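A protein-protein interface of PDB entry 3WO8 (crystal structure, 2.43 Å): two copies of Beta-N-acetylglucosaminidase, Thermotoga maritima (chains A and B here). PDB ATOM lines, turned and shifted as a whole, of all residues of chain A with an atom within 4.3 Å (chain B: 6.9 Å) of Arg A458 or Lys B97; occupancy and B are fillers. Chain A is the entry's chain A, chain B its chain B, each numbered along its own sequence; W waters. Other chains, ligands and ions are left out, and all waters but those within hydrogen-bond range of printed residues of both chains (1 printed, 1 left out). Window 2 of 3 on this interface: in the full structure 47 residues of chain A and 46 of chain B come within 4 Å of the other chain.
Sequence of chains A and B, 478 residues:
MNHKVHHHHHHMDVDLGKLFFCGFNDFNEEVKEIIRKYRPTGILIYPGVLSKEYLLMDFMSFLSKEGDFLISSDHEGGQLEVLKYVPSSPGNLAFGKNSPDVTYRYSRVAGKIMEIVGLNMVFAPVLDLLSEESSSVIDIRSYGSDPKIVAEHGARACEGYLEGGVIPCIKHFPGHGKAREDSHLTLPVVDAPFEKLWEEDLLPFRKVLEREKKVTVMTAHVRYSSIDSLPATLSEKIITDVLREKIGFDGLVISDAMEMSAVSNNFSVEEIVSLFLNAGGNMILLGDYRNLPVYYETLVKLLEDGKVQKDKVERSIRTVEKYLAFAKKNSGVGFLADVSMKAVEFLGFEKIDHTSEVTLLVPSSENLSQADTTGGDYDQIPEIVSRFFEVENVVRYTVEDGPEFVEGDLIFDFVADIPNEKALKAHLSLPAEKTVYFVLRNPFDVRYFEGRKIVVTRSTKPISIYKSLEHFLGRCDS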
ATOM      1  N   LYS A 342     -14.841 -30.272   7.936  1.00  0.00           N
ATOM      2  CA  LYS A 342     -16.241 -30.633   7.779  1.00  0.00           C
ATOM      3  C   LYS A 342     -17.158 -29.479   8.139  1.00  0.00           C
ATOM      4  O   LYS A 342     -18.245 -29.389   7.625  1.00  0.00           O
ATOM      5  CB  LYS A 342     -16.588 -31.868   8.598  1.00  0.00           C
ATOM      6  CG  LYS A 342     -17.872 -32.531   8.135  1.00  0.00           C
ATOM      7  CD  LYS A 342     -18.003 -33.920   8.755  1.00  0.00           C
ATOM      8  CE  LYS A 342     -19.413 -34.473   8.670  1.00  0.00           C
ATOM      9  NZ  LYS A 342     -19.534 -35.732   9.463  1.00  0.00           N
ATOM     10  N   ALA A 343     -16.720 -28.570   8.997  1.00  0.00           N
ATOM     11  CA  ALA A 343     -17.558 -27.437   9.350  1.00  0.00           C
ATOM     12  C   ALA A 343     -17.547 -26.352   8.324  1.00  0.00           C
ATOM     13  O   ALA A 343     -18.346 -25.440   8.422  1.00  0.00           O
ATOM     14  CB  ALA A 343     -17.141 -26.849  10.680  1.00  0.00           C
ATOM     15  N   GLU A 345     -18.128 -24.333   4.833  1.00  0.00           N
ATOM     16  CA  GLU A 345     -18.998 -24.246   3.662  1.00  0.00           C
ATOM     17  C   GLU A 345     -18.447 -23.239   2.634  1.00  0.00           C
ATOM     18  O   GLU A 345     -17.967 -22.146   2.995  1.00  0.00           O
ATOM     19  CB  GLU A 345     -20.405 -23.780   4.068  1.00  0.00           C
ATOM     20  CG  GLU A 345     -21.232 -24.779   4.863  1.00  0.00           C
ATOM     21  CD  GLU A 345     -22.702 -24.369   4.945  1.00  0.00           C
ATOM     22  OE1 GLU A 345     -22.993 -23.141   4.967  1.00  0.00           O
ATOM     23  OE2 GLU A 345     -23.570 -25.278   4.978  1.00  0.00           O
ATOM     24  N   LEU A 440     -16.091 -15.695   9.324  1.00  0.00           N
ATOM     25  CA  LEU A 440     -15.340 -16.438  10.364  1.00  0.00           C
ATOM     26  C   LEU A 440     -16.143 -16.825  11.622  1.00  0.00           C
ATOM     27  O   LEU A 440     -15.831 -17.841  12.271  1.00  0.00           O
ATOM     28  CB  LEU A 440     -14.078 -15.677  10.792  1.00  0.00           C
ATOM     29  CG  LEU A 440     -12.952 -15.527   9.764  1.00  0.00           C
ATOM     30  CD1 LEU A 440     -11.713 -14.841  10.356  1.00  0.00           C
ATOM     31  CD2 LEU A 440     -12.569 -16.888   9.199  1.00  0.00           C
ATOM     32  N   VAL A 456     -17.565 -20.045   4.615  1.00  0.00           N
ATOM     33  CA  VAL A 456     -18.001 -20.103   5.972  1.00  0.00           C
ATOM     34  C   VAL A 456     -17.218 -21.165   6.698  1.00  0.00           C
ATOM     35  O   VAL A 456     -17.496 -22.352   6.571  1.00  0.00           O
ATOM     36  CB  VAL A 456     -19.491 -20.387   6.085  1.00  0.00           C
ATOM     37  CG1 VAL A 456     -19.934 -20.282   7.542  1.00  0.00           C
ATOM     38  CG2 VAL A 456     -20.250 -19.400   5.228  1.00  0.00           C
ATOM     39  N   THR A 457     -16.241 -20.706   7.458  1.00  0.00           N
ATOM     40  CA  THR A 457     -15.663 -21.482   8.526  1.00  0.00           C
ATOM     41  C   THR A 457     -16.658 -21.323   9.673  1.00  0.00           C
ATOM     42  O   THR A 457     -17.493 -20.392   9.676  1.00  0.00           O
ATOM     43  CB  THR A 457     -14.307 -20.883   8.922  1.00  0.00           C
ATOM     44  OG1 THR A 457     -14.503 -19.577   9.431  1.00  0.00           O
ATOM     45  CG2 THR A 457     -13.396 -20.732   7.720  1.00  0.00           C
ATOM     46  N   ARG A 458     -16.601 -22.177  10.668  1.00  0.00           N
ATOM     47  CA  ARG A 458     -17.345 -21.847  11.882  1.00  0.00           C
ATOM     48  C   ARG A 458     -16.332 -21.627  13.014  1.00  0.00           C
ATOM     49  O   ARG A 458     -16.483 -22.153  14.135  1.00  0.00           O
ATOM     50  CB  ARG A 458     -18.337 -22.955  12.222  1.00  0.00           C
ATOM     51  CG  ARG A 458     -19.640 -22.841  11.480  1.00  0.00           C
ATOM     52  CD  ARG A 458     -20.356 -24.183  11.346  1.00  0.00           C
ATOM     53  NE  ARG A 458     -21.583 -24.036  10.570  1.00  0.00           N
ATOM     54  CZ  ARG A 458     -21.606 -23.847   9.254  1.00  0.00           C
ATOM     55  NH1 ARG A 458     -20.486 -23.800   8.548  1.00  0.00           N
ATOM     56  NH2 ARG A 458     -22.746 -23.693   8.629  1.00  0.00           N
ATOM     57  N   SER A 459     -15.271 -20.886  12.690  1.00  0.00           N
ATOM     58  CA  SER A 459     -14.204 -20.609  13.640  1.00  0.00           C
ATOM     59  C   SER A 459     -13.179 -19.675  13.021  1.00  0.00           C
ATOM     60  O   SER A 459     -13.093 -19.504  11.789  1.00  0.00           O
ATOM     61  CB  SER A 459     -13.559 -21.905  14.209  1.00  0.00           C
ATOM     62  OG  SER A 459     -12.206 -22.097  13.886  1.00  0.00           O
ATOM     63  N   PRO B  90     -11.025 -26.217  16.919  1.00  0.00           N
ATOM     64  CA  PRO B  90     -11.649 -25.093  16.278  1.00  0.00           C
ATOM     65  C   PRO B  90     -12.799 -24.477  17.060  1.00  0.00           C
ATOM     66  O   PRO B  90     -13.219 -23.389  16.685  1.00  0.00           O
ATOM     67  CB  PRO B  90     -12.118 -25.654  14.949  1.00  0.00           C
ATOM     68  CG  PRO B  90     -12.272 -27.114  15.196  1.00  0.00           C
ATOM     69  CD  PRO B  90     -11.235 -27.476  16.207  1.00  0.00           C
ATOM     70  N   GLY B  91     -13.295 -25.137  18.115  1.00  0.00           N
ATOM     71  CA  GLY B  91     -14.478 -24.664  18.847  1.00  0.00           C
ATOM     72  C   GLY B  91     -15.862 -25.344  18.598  1.00  0.00           C
ATOM     73  O   GLY B  91     -16.163 -25.862  17.503  1.00  0.00           O
ATOM     74  N   ASN B  92     -16.713 -25.294  19.627  1.00  0.00           N
ATOM     75  CA  ASN B  92     -18.046 -25.893  19.640  1.00  0.00           C
ATOM     76  C   ASN B  92     -18.926 -25.668  18.406  1.00  0.00           C
ATOM     77  O   ASN B  92     -19.683 -26.537  18.037  1.00  0.00           O
ATOM     78  CB  ASN B  92     -18.817 -25.413  20.863  1.00  0.00           C
ATOM     79  CG  ASN B  92     -18.246 -25.934  22.171  1.00  0.00           C
ATOM     80  OD1 ASN B  92     -17.257 -26.643  22.182  1.00  0.00           O
ATOM     81  ND2 ASN B  92     -18.888 -25.579  23.290  1.00  0.00           N
ATOM     82  N   LEU B  93     -18.861 -24.514  17.773  1.00  0.00           N
ATOM     83  CA  LEU B  93     -19.692 -24.288  16.589  1.00  0.00           C
ATOM     84  C   LEU B  93     -19.219 -25.195  15.448  1.00  0.00           C
ATOM     85  O   LEU B  93     -20.000 -25.917  14.827  1.00  0.00           O
ATOM     86  CB  LEU B  93     -19.673 -22.822  16.175  1.00  0.00           C
ATOM     87  CG  LEU B  93     -20.741 -22.442  15.147  1.00  0.00           C
ATOM     88  CD1 LEU B  93     -22.136 -22.667  15.719  1.00  0.00           C
ATOM     89  CD2 LEU B  93     -20.594 -21.005  14.644  1.00  0.00           C
ATOM     90  N   ALA B  94     -17.929 -25.192  15.204  1.00  0.00           N
ATOM     91  CA  ALA B  94     -17.341 -26.163  14.287  1.00  0.00           C
ATOM     92  C   ALA B  94     -17.718 -27.616  14.633  1.00  0.00           C
ATOM     93  O   ALA B  94     -18.120 -28.378  13.784  1.00  0.00           O
ATOM     94  CB  ALA B  94     -15.825 -25.997  14.260  1.00  0.00           C
ATOM     95  N   PHE B  95     -17.567 -27.982  15.886  1.00  0.00           N
ATOM     96  CA  PHE B  95     -17.844 -29.331  16.319  1.00  0.00           C
ATOM     97  C   PHE B  95     -19.322 -29.694  16.188  1.00  0.00           C
ATOM     98  O   PHE B  95     -19.669 -30.875  16.058  1.00  0.00           O
ATOM     99  CB  PHE B  95     -17.413 -29.511  17.788  1.00  0.00           C
ATOM    100  CG  PHE B  95     -16.033 -30.087  17.955  1.00  0.00           C
ATOM    101  CD1 PHE B  95     -15.819 -31.431  17.824  1.00  0.00           C
ATOM    102  CD2 PHE B  95     -14.968 -29.292  18.268  1.00  0.00           C
ATOM    103  CE1 PHE B  95     -14.558 -31.984  18.002  1.00  0.00           C
ATOM    104  CE2 PHE B  95     -13.710 -29.825  18.458  1.00  0.00           C
ATOM    105  CZ  PHE B  95     -13.502 -31.173  18.318  1.00  0.00           C
ATOM    106  N   GLY B  96     -20.179 -28.682  16.270  1.00  0.00           N
ATOM    107  CA  GLY B  96     -21.607 -28.850  16.108  1.00  0.00           C
ATOM    108  C   GLY B  96     -22.024 -29.326  14.722  1.00  0.00           C
ATOM    109  O   GLY B  96     -23.110 -29.860  14.543  1.00  0.00           O
ATOM    110  N   LYS B  97     -21.170 -29.151  13.737  1.00  0.00           N
ATOM    111  CA  LYS B  97     -21.457 -29.703  12.432  1.00  0.00           C
ATOM    112  C   LYS B  97     -20.749 -31.049  12.240  1.00  0.00           C
ATOM    113  O   LYS B  97     -20.588 -31.524  11.126  1.00  0.00           O
ATOM    114  CB  LYS B  97     -21.078 -28.703  11.349  1.00  0.00           C
ATOM    115  CG  LYS B  97     -22.025 -27.518  11.291  1.00  0.00           C
ATOM    116  CD  LYS B  97     -23.260 -27.807  10.449  1.00  0.00           C
ATOM    117  CE  LYS B  97     -24.410 -26.841  10.769  1.00  0.00           C
ATOM    118  NZ  LYS B  97     -25.350 -26.654   9.623  1.00  0.00           N
ATOM    119  N   ASN B  98     -20.357 -31.682  13.338  1.00  0.00           N
ATOM    120  CA  ASN B  98     -19.627 -32.950  13.289  1.00  0.00           C
ATOM    121  C   ASN B  98     -20.350 -34.029  14.091  1.00  0.00           C
ATOM    122  O   ASN B  98     -21.241 -33.761  14.884  1.00  0.00           O
ATOM    123  CB  ASN B  98     -18.202 -32.781  13.834  1.00  0.00           C
ATOM    124  CG  ASN B  98     -17.241 -32.209  12.808  1.00  0.00           C
ATOM    125  OD1 ASN B  98     -16.476 -32.943  12.179  1.00  0.00           O
ATOM    126  ND2 ASN B  98     -17.276 -30.894  12.634  1.00  0.00           N
ATOM    127  N   SER B  99     -19.965 -35.266  13.886  1.00  0.00           N
ATOM    128  CA  SER B  99     -20.498 -36.296  14.723  1.00  0.00           C
ATOM    129  C   SER B  99     -20.221 -35.926  16.198  1.00  0.00           C
ATOM    130  O   SER B  99     -19.132 -35.463  16.549  1.00  0.00           O
ATOM    131  CB  SER B  99     -19.888 -37.654  14.367  1.00  0.00           C
ATOM    132  OG  SER B  99     -20.085 -38.570  15.436  1.00  0.00           O
ATOM    133  N   ASP B 139     -21.532 -16.879  19.899  1.00  0.00           N
ATOM    134  CA  ASP B 139     -21.627 -17.510  18.576  1.00  0.00           C
ATOM    135  C   ASP B 139     -20.691 -18.728  18.361  1.00  0.00           C
ATOM    136  O   ASP B 139     -21.177 -19.875  18.333  1.00  0.00           O
ATOM    137  CB  ASP B 139     -21.536 -16.483  17.402  1.00  0.00           C
ATOM    138  CG  ASP B 139     -20.328 -15.539  17.487  1.00  0.00           C
ATOM    139  OD1 ASP B 139     -19.208 -16.025  17.777  1.00  0.00           O
ATOM    140  OD2 ASP B 139     -20.502 -14.316  17.219  1.00  0.00           O
ATOM    141  N   ILE B 140     -19.375 -18.505  18.233  1.00  0.00           N
ATOM    142  CA  ILE B 140     -18.448 -19.632  18.008  1.00  0.00           C
ATOM    143  C   ILE B 140     -18.236 -20.516  19.218  1.00  0.00           C
ATOM    144  O   ILE B 140     -17.794 -21.644  19.061  1.00  0.00           O
ATOM    145  CB  ILE B 140     -17.066 -19.242  17.442  1.00  0.00           C
ATOM    146  CG1 ILE B 140     -16.297 -18.290  18.372  1.00  0.00           C
ATOM    147  CG2 ILE B 140     -17.230 -18.632  16.063  1.00  0.00           C
ATOM    148  CD1 ILE B 140     -14.803 -18.257  18.102  1.00  0.00           C
ATOM    149  N   TYR B 143     -22.365 -24.771  20.565  1.00  0.00           N
ATOM    150  CA  TYR B 143     -22.488 -25.844  19.596  1.00  0.00           C
ATOM    151  C   TYR B 143     -23.322 -25.450  18.391  1.00  0.00           C
ATOM    152  O   TYR B 143     -23.055 -25.932  17.304  1.00  0.00           O
ATOM    153  CB  TYR B 143     -23.070 -27.084  20.252  1.00  0.00           C
ATOM    154  CG  TYR B 143     -22.090 -27.750  21.166  1.00  0.00           C
ATOM    155  CD1 TYR B 143     -20.938 -28.334  20.652  1.00  0.00           C
ATOM    156  CD2 TYR B 143     -22.288 -27.767  22.546  1.00  0.00           C
ATOM    157  CE1 TYR B 143     -20.027 -28.953  21.485  1.00  0.00           C
ATOM    158  CE2 TYR B 143     -21.384 -28.369  23.390  1.00  0.00           C
ATOM    159  CZ  TYR B 143     -20.253 -28.968  22.854  1.00  0.00           C
ATOM    160  OH  TYR B 143     -19.329 -29.595  23.672  1.00  0.00           O
ATOM    161  N   ILE B 149     -29.155 -30.692  18.735  1.00  0.00           N
ATOM    162  CA  ILE B 149     -27.739 -30.845  18.449  1.00  0.00           C
ATOM    163  C   ILE B 149     -26.856 -30.462  19.645  1.00  0.00           C
ATOM    164  O   ILE B 149     -25.911 -31.188  20.054  1.00  0.00           O
ATOM    165  CB  ILE B 149     -27.393 -30.001  17.225  1.00  0.00           C
ATOM    166  CG1 ILE B 149     -28.001 -30.654  15.981  1.00  0.00           C
ATOM    167  CG2 ILE B 149     -25.890 -29.909  17.052  1.00  0.00           C
ATOM    168  CD1 ILE B 149     -27.967 -29.780  14.739  1.00  0.00           C
ATOM    169  N   HIS B 153     -24.216 -32.912  21.669  1.00  0.00           N
ATOM    170  CA  HIS B 153     -22.809 -32.590  21.810  1.00  0.00           C
ATOM    171  C   HIS B 153     -22.448 -32.336  23.275  1.00  0.00           C
ATOM    172  O   HIS B 153     -21.415 -32.829  23.765  1.00  0.00           O
ATOM    173  CB  HIS B 153     -22.449 -31.449  20.906  1.00  0.00           C
ATOM    174  CG  HIS B 153     -22.401 -31.841  19.467  1.00  0.00           C
ATOM    175  ND1 HIS B 153     -23.520 -31.870  18.667  1.00  0.00           N
ATOM    176  CD2 HIS B 153     -21.368 -32.215  18.676  1.00  0.00           C
ATOM    177  CE1 HIS B 153     -23.178 -32.228  17.441  1.00  0.00           C
ATOM    178  NE2 HIS B 153     -21.877 -32.445  17.420  1.00  0.00           N
HETATM  179  O   HOH W   1     -17.726 -36.237  11.889  1.00  0.00           O
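The backbone carbonyl oxygen (O) of Pro B90 sits close to the side-chain hydroxyl (OG) of Ser A459 (3.2 Å).
A ring nitrogen (NE2) of His B153 is in hydrogen-bond range of the backbone carbonyl oxygen of Asn B98 (2.9 Å). The backbone NH (N) of Ser A459 is in hydrogen-bond range of the backbone carbonyl oxygen (O) of Leu A440. The backbone carbonyl oxygen (O) of Ala A343 lies within hydrogen-bond range of the guanidinium group (NH1) of Arg A458, at 2.7 Å. The backbone NH of Leu B93 is in hydrogen-bond range of the backbone carbonyl oxygen of Ile B140 (3.3 Å). The side-chain carboxylate of Glu A345 is in salt-bridge range of the guanidinium group of Arg A458 (3.7 Å). ND2 of Asn B98 sits at hydrogen-bond distance from O of Ala B94, 2.9 Å away.
Lys A342 touches Asn B98. CB of Ala A343 touches O of Ala B94, 3.6 Å away. Arg A458 touches Leu B93 (CG to CD2, 3.8 Å). Arg A458 touches Ala B94 (O to N, 3.5 Å). Arg A458 touches Lys B97 (NE to CG, 3.6 Å).
Arg A458 touches just these residues of chain B: Leu B93, Ala B94 and Lys B97. Of the printed residues of chain A, Lys B97 touches Arg A458 (3.6 Å). Of the printed residues of chain B, Lys A342 touches Asn B98. Of the printed residues of chain A, Pro B90 touches Ser A459. The nearest residue of chain B that does not touch Arg A458 is Ile B140 (4.1 Å). The nearest printed residue of chain A that does not touch Ala B94 is Ser A459 (4.7 Å).
Hydrophobic or aromatic side chains of chain A that line the printed part of chain B: Ala A343. Along chain A the printed residues that touch a printed residue of chain B span positions 342 to 459. Of the 15 printed residues of chain B, 5 touch a printed residue of chain A. Hydrophobic or aromatic side chains of chain B that line the printed part of chain A: Pro B90, Leu B93 and Ala B94. Along chain B the printed residues that touch a printed residue of chain A span positions 90 to 98. Among the printed residues, 6 pairs touch across the chains. Among the printed residues, no Asp or Glu carboxylate lies within 4 Å of a Lys or Arg side-chain nitrogen of the other chain.
No position is printed for both chains. Of the 6 pairs that touch across the chains among the printed residues, none has its exchanged pair printed and touching as well.
Water W1 lies within hydrogen-bond range of NZ of Lys A342 (3.1 Å) and N of Ser B99 (3.2 Å).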
